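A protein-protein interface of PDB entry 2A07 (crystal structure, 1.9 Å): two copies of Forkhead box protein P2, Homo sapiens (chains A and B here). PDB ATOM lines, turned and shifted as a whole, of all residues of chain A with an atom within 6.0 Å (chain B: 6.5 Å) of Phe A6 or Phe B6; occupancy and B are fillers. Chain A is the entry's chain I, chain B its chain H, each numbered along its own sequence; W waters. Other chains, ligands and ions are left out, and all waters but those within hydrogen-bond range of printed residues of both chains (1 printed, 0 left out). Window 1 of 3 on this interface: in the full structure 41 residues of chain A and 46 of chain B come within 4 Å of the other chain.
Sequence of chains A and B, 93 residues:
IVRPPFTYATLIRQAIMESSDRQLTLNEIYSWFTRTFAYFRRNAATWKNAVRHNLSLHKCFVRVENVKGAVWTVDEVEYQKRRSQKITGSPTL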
ATOM      1  N   PRO A   4     -13.258  22.393  12.118  1.00  0.00           N
ATOM      2  CA  PRO A   4     -14.064  21.188  12.335  1.00  0.00           C
ATOM      3  C   PRO A   4     -15.543  21.544  12.522  1.00  0.00           C
ATOM      4  O   PRO A   4     -15.870  22.593  13.073  1.00  0.00           O
ATOM      5  CB  PRO A   4     -13.458  20.589  13.604  1.00  0.00           C
ATOM      6  CG  PRO A   4     -12.038  21.078  13.573  1.00  0.00           C
ATOM      7  CD  PRO A   4     -12.208  22.508  13.144  1.00  0.00           C
ATOM      8  N   PRO A   5     -16.454  20.679  12.054  1.00  0.00           N
ATOM      9  CA  PRO A   5     -17.891  20.948  12.200  1.00  0.00           C
ATOM     10  C   PRO A   5     -18.270  21.151  13.669  1.00  0.00           C
ATOM     11  O   PRO A   5     -19.096  22.005  13.996  1.00  0.00           O
ATOM     12  CB  PRO A   5     -18.535  19.696  11.611  1.00  0.00           C
ATOM     13  CG  PRO A   5     -17.554  19.281  10.563  1.00  0.00           C
ATOM     14  CD  PRO A   5     -16.227  19.455  11.268  1.00  0.00           C
ATOM     15  N   PHE A   6     -17.654  20.361  14.548  1.00  0.00           N
ATOM     16  CA  PHE A   6     -17.905  20.446  15.983  1.00  0.00           C
ATOM     17  C   PHE A   6     -16.619  20.230  16.777  1.00  0.00           C
ATOM     18  O   PHE A   6     -15.679  19.599  16.295  1.00  0.00           O
ATOM     19  CB  PHE A   6     -18.916  19.374  16.433  1.00  0.00           C
ATOM     20  CG  PHE A   6     -20.251  19.456  15.736  1.00  0.00           C
ATOM     21  CD1 PHE A   6     -20.440  18.853  14.499  1.00  0.00           C
ATOM     22  CD2 PHE A   6     -21.308  20.154  16.312  1.00  0.00           C
ATOM     23  CE1 PHE A   6     -21.666  18.936  13.839  1.00  0.00           C
ATOM     24  CE2 PHE A   6     -22.545  20.244  15.657  1.00  0.00           C
ATOM     25  CZ  PHE A   6     -22.718  19.632  14.418  1.00  0.00           C
ATOM     26  N   THR A   7     -16.598  20.759  17.995  1.00  0.00           N
ATOM     27  CA  THR A   7     -15.475  20.581  18.908  1.00  0.00           C
ATOM     28  C   THR A   7     -16.151  20.428  20.258  1.00  0.00           C
ATOM     29  O   THR A   7     -17.339  20.741  20.388  1.00  0.00           O
ATOM     30  CB  THR A   7     -14.547  21.817  18.946  1.00  0.00           C
ATOM     31  OG1 THR A   7     -15.235  22.915  19.553  1.00  0.00           O
ATOM     32  CG2 THR A   7     -14.144  22.208  17.546  1.00  0.00           C
ATOM     33  N   TYR A   8     -15.430  19.951  21.265  1.00  0.00           N
ATOM     34  CA  TYR A   8     -16.056  19.803  22.566  1.00  0.00           C
ATOM     35  C   TYR A   8     -16.530  21.168  23.035  1.00  0.00           C
ATOM     36  O   TYR A   8     -17.592  21.288  23.654  1.00  0.00           O
ATOM     37  CB  TYR A   8     -15.086  19.193  23.580  1.00  0.00           C
ATOM     38  CG  TYR A   8     -14.754  17.754  23.250  1.00  0.00           C
ATOM     39  CD1 TYR A   8     -13.520  17.411  22.685  1.00  0.00           C
ATOM     40  CD2 TYR A   8     -15.692  16.738  23.458  1.00  0.00           C
ATOM     41  CE1 TYR A   8     -13.228  16.094  22.334  1.00  0.00           C
ATOM     42  CE2 TYR A   8     -15.407  15.401  23.108  1.00  0.00           C
ATOM     43  CZ  TYR A   8     -14.174  15.094  22.552  1.00  0.00           C
ATOM     44  OH  TYR A   8     -13.848  13.789  22.231  1.00  0.00           O
ATOM     45  N   THR A  10     -17.607  23.843  21.174  1.00  0.00           N
ATOM     46  CA  THR A  10     -18.858  24.298  20.566  1.00  0.00           C
ATOM     47  C   THR A  10     -20.051  23.491  21.075  1.00  0.00           C
ATOM     48  O   THR A  10     -21.141  24.032  21.241  1.00  0.00           O
ATOM     49  CB  THR A  10     -18.829  24.261  19.010  1.00  0.00           C
ATOM     50  OG1 THR A  10     -18.734  22.914  18.545  1.00  0.00           O
ATOM     51  CG2 THR A  10     -17.637  25.044  18.475  1.00  0.00           C
ATOM     52  N   LEU A  11     -19.838  22.206  21.351  1.00  0.00           N
ATOM     53  CA  LEU A  11     -20.908  21.343  21.849  1.00  0.00           C
ATOM     54  C   LEU A  11     -21.292  21.684  23.285  1.00  0.00           C
ATOM     55  O   LEU A  11     -22.471  21.690  23.632  1.00  0.00           O
ATOM     56  CB  LEU A  11     -20.493  19.872  21.753  1.00  0.00           C
ATOM     57  CG  LEU A  11     -20.426  19.314  20.331  1.00  0.00           C
ATOM     58  CD1 LEU A  11     -19.717  17.970  20.345  1.00  0.00           C
ATOM     59  CD2 LEU A  11     -21.839  19.181  19.765  1.00  0.00           C
ATOM     60  N   GLN A  14     -23.279  24.824  23.121  1.00  0.00           N
ATOM     61  CA  GLN A  14     -24.630  24.583  22.624  1.00  0.00           C
ATOM     62  C   GLN A  14     -25.523  24.041  23.744  1.00  0.00           C
ATOM     63  O   GLN A  14     -26.622  24.548  23.978  1.00  0.00           O
ATOM     64  CB  GLN A  14     -24.607  23.582  21.465  1.00  0.00           C
ATOM     65  CG  GLN A  14     -25.902  23.553  20.649  1.00  0.00           C
ATOM     66  CD  GLN A  14     -25.898  22.468  19.586  1.00  0.00           C
ATOM     67  OE1 GLN A  14     -24.873  22.206  18.955  1.00  0.00           O
ATOM     68  NE2 GLN A  14     -27.051  21.839  19.375  1.00  0.00           N
ATOM     69  N   TRP A  32     -26.737  15.466  28.147  1.00  0.00           N
ATOM     70  CA  TRP A  32     -26.860  16.067  26.826  1.00  0.00           C
ATOM     71  C   TRP A  32     -25.902  15.371  25.854  1.00  0.00           C
ATOM     72  O   TRP A  32     -26.284  15.027  24.738  1.00  0.00           O
ATOM     73  CB  TRP A  32     -26.539  17.565  26.898  1.00  0.00           C
ATOM     74  CG  TRP A  32     -26.828  18.324  25.628  1.00  0.00           C
ATOM     75  CD1 TRP A  32     -27.994  18.966  25.302  1.00  0.00           C
ATOM     76  CD2 TRP A  32     -25.940  18.518  24.518  1.00  0.00           C
ATOM     77  NE1 TRP A  32     -27.885  19.543  24.063  1.00  0.00           N
ATOM     78  CE2 TRP A  32     -26.638  19.282  23.556  1.00  0.00           C
ATOM     79  CE3 TRP A  32     -24.628  18.111  24.238  1.00  0.00           C
ATOM     80  CZ2 TRP A  32     -26.065  19.658  22.337  1.00  0.00           C
ATOM     81  CZ3 TRP A  32     -24.058  18.483  23.020  1.00  0.00           C
ATOM     82  CH2 TRP A  32     -24.777  19.245  22.085  1.00  0.00           C
ATOM     83  N   THR A  36     -26.662  13.225  22.496  1.00  0.00           N
ATOM     84  CA  THR A  36     -26.064  13.671  21.250  1.00  0.00           C
ATOM     85  C   THR A  36     -25.228  12.580  20.568  1.00  0.00           C
ATOM     86  O   THR A  36     -25.398  12.317  19.379  1.00  0.00           O
ATOM     87  CB  THR A  36     -25.209  14.937  21.487  1.00  0.00           C
ATOM     88  OG1 THR A  36     -26.073  16.011  21.893  1.00  0.00           O
ATOM     89  CG2 THR A  36     -24.463  15.338  20.208  1.00  0.00           C
ATOM     90  N   TYR A  39     -27.424  10.000  18.978  1.00  0.00           N
ATOM     91  CA  TYR A  39     -28.037  10.432  17.725  1.00  0.00           C
ATOM     92  C   TYR A  39     -27.114  10.173  16.538  1.00  0.00           C
ATOM     93  O   TYR A  39     -27.554   9.715  15.483  1.00  0.00           O
ATOM     94  CB  TYR A  39     -28.378  11.928  17.777  1.00  0.00           C
ATOM     95  CG  TYR A  39     -28.996  12.465  16.504  1.00  0.00           C
ATOM     96  CD1 TYR A  39     -30.372  12.353  16.262  1.00  0.00           C
ATOM     97  CD2 TYR A  39     -28.209  13.079  15.533  1.00  0.00           C
ATOM     98  CE1 TYR A  39     -30.938  12.846  15.076  1.00  0.00           C
ATOM     99  CE2 TYR A  39     -28.763  13.570  14.350  1.00  0.00           C
ATOM    100  CZ  TYR A  39     -30.134  13.448  14.132  1.00  0.00           C
ATOM    101  OH  TYR A  39     -30.666  13.943  12.968  1.00  0.00           O
ATOM    102  N   PHE A  40     -25.828  10.462  16.711  1.00  0.00           N
ATOM    103  CA  PHE A  40     -24.868  10.280  15.623  1.00  0.00           C
ATOM    104  C   PHE A  40     -24.389   8.859  15.369  1.00  0.00           C
ATOM    105  O   PHE A  40     -23.667   8.611  14.402  1.00  0.00           O
ATOM    106  CB  PHE A  40     -23.671  11.214  15.831  1.00  0.00           C
ATOM    107  CG  PHE A  40     -24.005  12.655  15.594  1.00  0.00           C
ATOM    108  CD1 PHE A  40     -24.268  13.513  16.654  1.00  0.00           C
ATOM    109  CD2 PHE A  40     -24.118  13.143  14.295  1.00  0.00           C
ATOM    110  CE1 PHE A  40     -24.637  14.839  16.422  1.00  0.00           C
ATOM    111  CE2 PHE A  40     -24.486  14.463  14.054  1.00  0.00           C
ATOM    112  CZ  PHE A  40     -24.746  15.312  15.121  1.00  0.00           C
ATOM    113  N   PRO B   5     -32.361  19.246  19.469  1.00  0.00           N
ATOM    114  CA  PRO B   5     -30.894  19.446  19.400  1.00  0.00           C
ATOM    115  C   PRO B   5     -30.423  19.429  17.948  1.00  0.00           C
ATOM    116  O   PRO B   5     -29.995  20.453  17.413  1.00  0.00           O
ATOM    117  CB  PRO B   5     -30.256  18.318  20.199  1.00  0.00           C
ATOM    118  CG  PRO B   5     -31.329  17.232  20.092  1.00  0.00           C
ATOM    119  CD  PRO B   5     -32.662  17.992  20.183  1.00  0.00           C
ATOM    120  N   PHE B   6     -30.493  18.262  17.315  1.00  0.00           N
ATOM    121  CA  PHE B   6     -30.095  18.128  15.921  1.00  0.00           C
ATOM    122  C   PHE B   6     -31.122  17.315  15.146  1.00  0.00           C
ATOM    123  O   PHE B   6     -31.704  16.373  15.685  1.00  0.00           O
ATOM    124  CB  PHE B   6     -28.759  17.393  15.783  1.00  0.00           C
ATOM    125  CG  PHE B   6     -27.648  17.979  16.588  1.00  0.00           C
ATOM    126  CD1 PHE B   6     -27.436  17.581  17.902  1.00  0.00           C
ATOM    127  CD2 PHE B   6     -26.799  18.924  16.023  1.00  0.00           C
ATOM    128  CE1 PHE B   6     -26.383  18.119  18.650  1.00  0.00           C
ATOM    129  CE2 PHE B   6     -25.746  19.470  16.760  1.00  0.00           C
ATOM    130  CZ  PHE B   6     -25.538  19.066  18.073  1.00  0.00           C
ATOM    131  N   THR B   7     -31.324  17.685  13.886  1.00  0.00           N
ATOM    132  CA  THR B   7     -32.209  16.963  12.978  1.00  0.00           C
ATOM    133  C   THR B   7     -31.426  17.020  11.686  1.00  0.00           C
ATOM    134  O   THR B   7     -30.460  17.783  11.587  1.00  0.00           O
ATOM    135  CB  THR B   7     -33.584  17.661  12.747  1.00  0.00           C
ATOM    136  OG1 THR B   7     -33.396  18.862  11.986  1.00  0.00           O
ATOM    137  CG2 THR B   7     -34.255  17.980  14.081  1.00  0.00           C
ATOM    138  N   TYR B   8     -31.807  16.230  10.692  1.00  0.00           N
ATOM    139  CA  TYR B   8     -31.066  16.277   9.450  1.00  0.00           C
ATOM    140  C   TYR B   8     -31.160  17.659   8.831  1.00  0.00           C
ATOM    141  O   TYR B   8     -30.221  18.124   8.185  1.00  0.00           O
ATOM    142  CB  TYR B   8     -31.562  15.206   8.475  1.00  0.00           C
ATOM    143  CG  TYR B   8     -30.963  13.863   8.795  1.00  0.00           C
ATOM    144  CD1 TYR B   8     -31.623  12.958   9.623  1.00  0.00           C
ATOM    145  CD2 TYR B   8     -29.682  13.535   8.345  1.00  0.00           C
ATOM    146  CE1 TYR B   8     -31.020  11.759   9.999  1.00  0.00           C
ATOM    147  CE2 TYR B   8     -29.072  12.346   8.715  1.00  0.00           C
ATOM    148  CZ  TYR B   8     -29.741  11.465   9.540  1.00  0.00           C
ATOM    149  OH  TYR B   8     -29.121  10.296   9.909  1.00  0.00           O
ATOM    150  N   ALA B   9     -32.291  18.320   9.049  1.00  0.00           N
ATOM    151  CA  ALA B   9     -32.495  19.656   8.506  1.00  0.00           C
ATOM    152  C   ALA B   9     -31.540  20.667   9.135  1.00  0.00           C
ATOM    153  O   ALA B   9     -30.931  21.461   8.419  1.00  0.00           O
ATOM    154  CB  ALA B   9     -33.952  20.106   8.712  1.00  0.00           C
ATOM    155  N   THR B  10     -31.402  20.646  10.459  1.00  0.00           N
ATOM    156  CA  THR B  10     -30.501  21.600  11.121  1.00  0.00           C
ATOM    157  C   THR B  10     -29.059  21.329  10.692  1.00  0.00           C
ATOM    158  O   THR B  10     -28.268  22.259  10.472  1.00  0.00           O
ATOM    159  CB  THR B  10     -30.587  21.528  12.679  1.00  0.00           C
ATOM    160  OG1 THR B  10     -29.994  20.311  13.159  1.00  0.00           O
ATOM    161  CG2 THR B  10     -32.040  21.601  13.138  1.00  0.00           C
ATOM    162  N   LEU B  11     -28.725  20.051  10.552  1.00  0.00           N
ATOM    163  CA  LEU B  11     -27.381  19.669  10.148  1.00  0.00           C
ATOM    164  C   LEU B  11     -27.082  20.082   8.715  1.00  0.00           C
ATOM    165  O   LEU B  11     -26.002  20.601   8.422  1.00  0.00           O
ATOM    166  CB  LEU B  11     -27.194  18.160  10.316  1.00  0.00           C
ATOM    167  CG  LEU B  11     -27.066  17.703  11.772  1.00  0.00           C
ATOM    168  CD1 LEU B  11     -27.063  16.183  11.840  1.00  0.00           C
ATOM    169  CD2 LEU B  11     -25.778  18.269  12.363  1.00  0.00           C
ATOM    170  N   GLN B  14     -26.554  23.717   8.792  1.00  0.00           N
ATOM    171  CA  GLN B  14     -25.265  24.050   9.386  1.00  0.00           C
ATOM    172  C   GLN B  14     -24.155  23.923   8.348  1.00  0.00           C
ATOM    173  O   GLN B  14     -23.301  24.811   8.225  1.00  0.00           O
ATOM    174  CB  GLN B  14     -24.963  23.129  10.571  1.00  0.00           C
ATOM    175  CG  GLN B  14     -23.827  23.633  11.457  1.00  0.00           C
ATOM    176  CD  GLN B  14     -23.444  22.658  12.562  1.00  0.00           C
ATOM    177  OE1 GLN B  14     -24.298  21.971  13.126  1.00  0.00           O
ATOM    178  NE2 GLN B  14     -22.150  22.611  12.889  1.00  0.00           N
ATOM    179  N   TRP B  32     -19.328  16.689   4.179  1.00  0.00           N
ATOM    180  CA  TRP B  32     -19.504  17.325   5.480  1.00  0.00           C
ATOM    181  C   TRP B  32     -20.105  16.328   6.476  1.00  0.00           C
ATOM    182  O   TRP B  32     -19.654  16.235   7.621  1.00  0.00           O
ATOM    183  CB  TRP B  32     -20.404  18.562   5.353  1.00  0.00           C
ATOM    184  CG  TRP B  32     -20.474  19.394   6.599  1.00  0.00           C
ATOM    185  CD1 TRP B  32     -19.686  20.464   6.922  1.00  0.00           C
ATOM    186  CD2 TRP B  32     -21.385  19.224   7.689  1.00  0.00           C
ATOM    187  NE1 TRP B  32     -20.054  20.975   8.145  1.00  0.00           N
ATOM    188  CE2 TRP B  32     -21.095  20.230   8.637  1.00  0.00           C
ATOM    189  CE3 TRP B  32     -22.417  18.318   7.956  1.00  0.00           C
ATOM    190  CZ2 TRP B  32     -21.808  20.357   9.838  1.00  0.00           C
ATOM    191  CZ3 TRP B  32     -23.127  18.443   9.152  1.00  0.00           C
ATOM    192  CH2 TRP B  32     -22.817  19.458  10.077  1.00  0.00           C
ATOM    193  N   THR B  36     -18.534  14.803   9.909  1.00  0.00           N
ATOM    194  CA  THR B  36     -19.296  14.934  11.142  1.00  0.00           C
ATOM    195  C   THR B  36     -19.556  13.612  11.852  1.00  0.00           C
ATOM    196  O   THR B  36     -19.300  13.482  13.051  1.00  0.00           O
ATOM    197  CB  THR B  36     -20.627  15.668  10.865  1.00  0.00           C
ATOM    198  OG1 THR B  36     -20.334  16.985  10.389  1.00  0.00           O
ATOM    199  CG2 THR B  36     -21.468  15.779  12.113  1.00  0.00           C
ATOM    200  N   TYR B  39     -16.396  12.207  13.379  1.00  0.00           N
ATOM    201  CA  TYR B  39     -16.039  12.838  14.647  1.00  0.00           C
ATOM    202  C   TYR B  39     -16.683  12.137  15.842  1.00  0.00           C
ATOM    203  O   TYR B  39     -16.005  11.801  16.819  1.00  0.00           O
ATOM    204  CB  TYR B  39     -16.463  14.315  14.647  1.00  0.00           C
ATOM    205  CG  TYR B  39     -16.218  15.038  15.959  1.00  0.00           C
ATOM    206  CD1 TYR B  39     -14.966  15.579  16.260  1.00  0.00           C
ATOM    207  CD2 TYR B  39     -17.235  15.163  16.910  1.00  0.00           C
ATOM    208  CE1 TYR B  39     -14.733  16.230  17.471  1.00  0.00           C
ATOM    209  CE2 TYR B  39     -17.012  15.806  18.123  1.00  0.00           C
ATOM    210  CZ  TYR B  39     -15.755  16.336  18.394  1.00  0.00           C
ATOM    211  OH  TYR B  39     -15.544  16.969  19.586  1.00  0.00           O
ATOM    212  N   PHE B  40     -17.995  11.921  15.781  1.00  0.00           N
ATOM    213  CA  PHE B  40     -18.674  11.283  16.896  1.00  0.00           C
ATOM    214  C   PHE B  40     -18.294   9.816  17.083  1.00  0.00           C
ATOM    215  O   PHE B  40     -18.279   9.317  18.207  1.00  0.00           O
ATOM    216  CB  PHE B  40     -20.195  11.462  16.759  1.00  0.00           C
ATOM    217  CG  PHE B  40     -20.637  12.885  16.943  1.00  0.00           C
ATOM    218  CD1 PHE B  40     -20.823  13.721  15.844  1.00  0.00           C
ATOM    219  CD2 PHE B  40     -20.761  13.420  18.221  1.00  0.00           C
ATOM    220  CE1 PHE B  40     -21.116  15.073  16.024  1.00  0.00           C
ATOM    221  CE2 PHE B  40     -21.054  14.780  18.411  1.00  0.00           C
ATOM    222  CZ  PHE B  40     -21.228  15.603  17.306  1.00  0.00           C
HETATM  223  O   HOH W   1     -13.145  18.436  19.601  1.00  0.00           O
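Pro A5 touches Trp B32 (CB to CZ2, 3.8 Å).
CZ of Phe A6 touches CD2 of Leu B11 (3.9 Å).
C of Thr A7 touches OH of Tyr B39, at 3.6 Å.
Leu A11 touches Phe B40.
O of Pro B5 touches NE2 of Gln A14 (3.8 Å).
Trp A32 touches Phe B6.
Thr A36 touches Phe B40 (CG2 to CE2, 3.9 Å).
Tyr A39 touches Thr B7.
Phe A40 touches Leu B11.
CG of Phe A40 touches CD1 of Phe B40 (3.4 Å).
Water W1 bridges the side-chain hydroxyl of Tyr B39 (2.8 Å) and the backbone NH of Tyr A8 (3.2 Å).
The side-chain hydroxyl of Thr B7 lies close to the backbone NH of Ala B9 (3.2 Å).
The backbone carbonyl oxygen of Trp A32 lies within hydrogen-bond range of the side-chain hydroxyl of Thr A36 (3.0 Å).
The backbone NH (N) of Thr A10 is in hydrogen-bond range of the side-chain hydroxyl (OG1) of Thr A7.
The side-chain hydroxyl (OG1) of Thr B36 is in hydrogen-bond range of the backbone carbonyl oxygen (O) of Trp B32, 2.9 Å away.
O of Thr B7 lies within hydrogen-bond range of OG1 of Thr B10 (3.0 Å).
Of chain B, only Phe B6 (3.5 Å), Leu B11 (3.9 Å), Gln B14 (3.1 Å), Trp B32 (3.97 Å), Thr B36 (3.6 Å) and Tyr B39 (3.7 Å) come within 4 Å of Phe A6.
Thr A10 touches none of the printed residues of chain B.
Printed residues of chain B within 4 Å of Thr A36: Phe B6 and Phe B40.
Printed residues of chain B within 4 Å of Tyr A39: Phe B6 (3.7 Å), Thr B7 (3.4 Å) and Tyr B8 (3.4 Å).
Printed residues of chain B within 4 Å of Phe A40: Leu B11 (3.8 Å), Thr B36 (3.8 Å) and Phe B40 (3.4 Å).
Of chain A, only Phe A6 (3.5 Å), Gln A14 (3.3 Å), Trp A32 (3.96 Å), Thr A36 (3.7 Å) and Tyr A39 (3.7 Å) come within 4 Å of Phe B6.
Ala B9 touches none of the printed residues of chain A.
Printed residues of chain A within 4 Å of Gln B14: Pro A5 and Phe A6.
The nearest residue of chain B that does not touch Phe A6 is Phe B40 (4.1 Å).
The nearest residue of chain A that does not touch Phe B6 is Leu A11 (4.1 Å).
The backbone NH (N) of Tyr B8 sits at hydrogen-bond distance from the side-chain hydroxyl (OH) of Tyr A39, 3.4 Å away.
The side-chain hydroxyl (OH) of Tyr B39 sits at hydrogen-bond distance from the backbone NH (N) of Tyr A8, at 3.4 Å.
The backbone carbonyl oxygen of Pro A5 is in hydrogen-bond range of the side-chain amide nitrogen of Gln B14.
Pro A5 touches Trp B32, but with the chains exchanged Trp A32 does not touch Pro B5 (4.7 Å).
Phe B6 touches its own counterpart, Phe A6.
Phe A6 touches Trp B32, and with the chains exchanged Trp A32 touches Phe B6.
Thr A36 touches Phe B40, and with the chains exchanged Phe A40 touches Thr B36.
Hydrophobic or aromatic side chains of chain B that line the printed part of chain A: Phe B6, Tyr B8, Leu B11, Trp B32, Tyr B39 and Phe B40.
Among the printed residues, 23 pairs touch across the chains.
Among the printed residues, no Asp or Glu carboxylate lies within 4 Å of a Lys or Arg side-chain nitrogen of the other chain.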
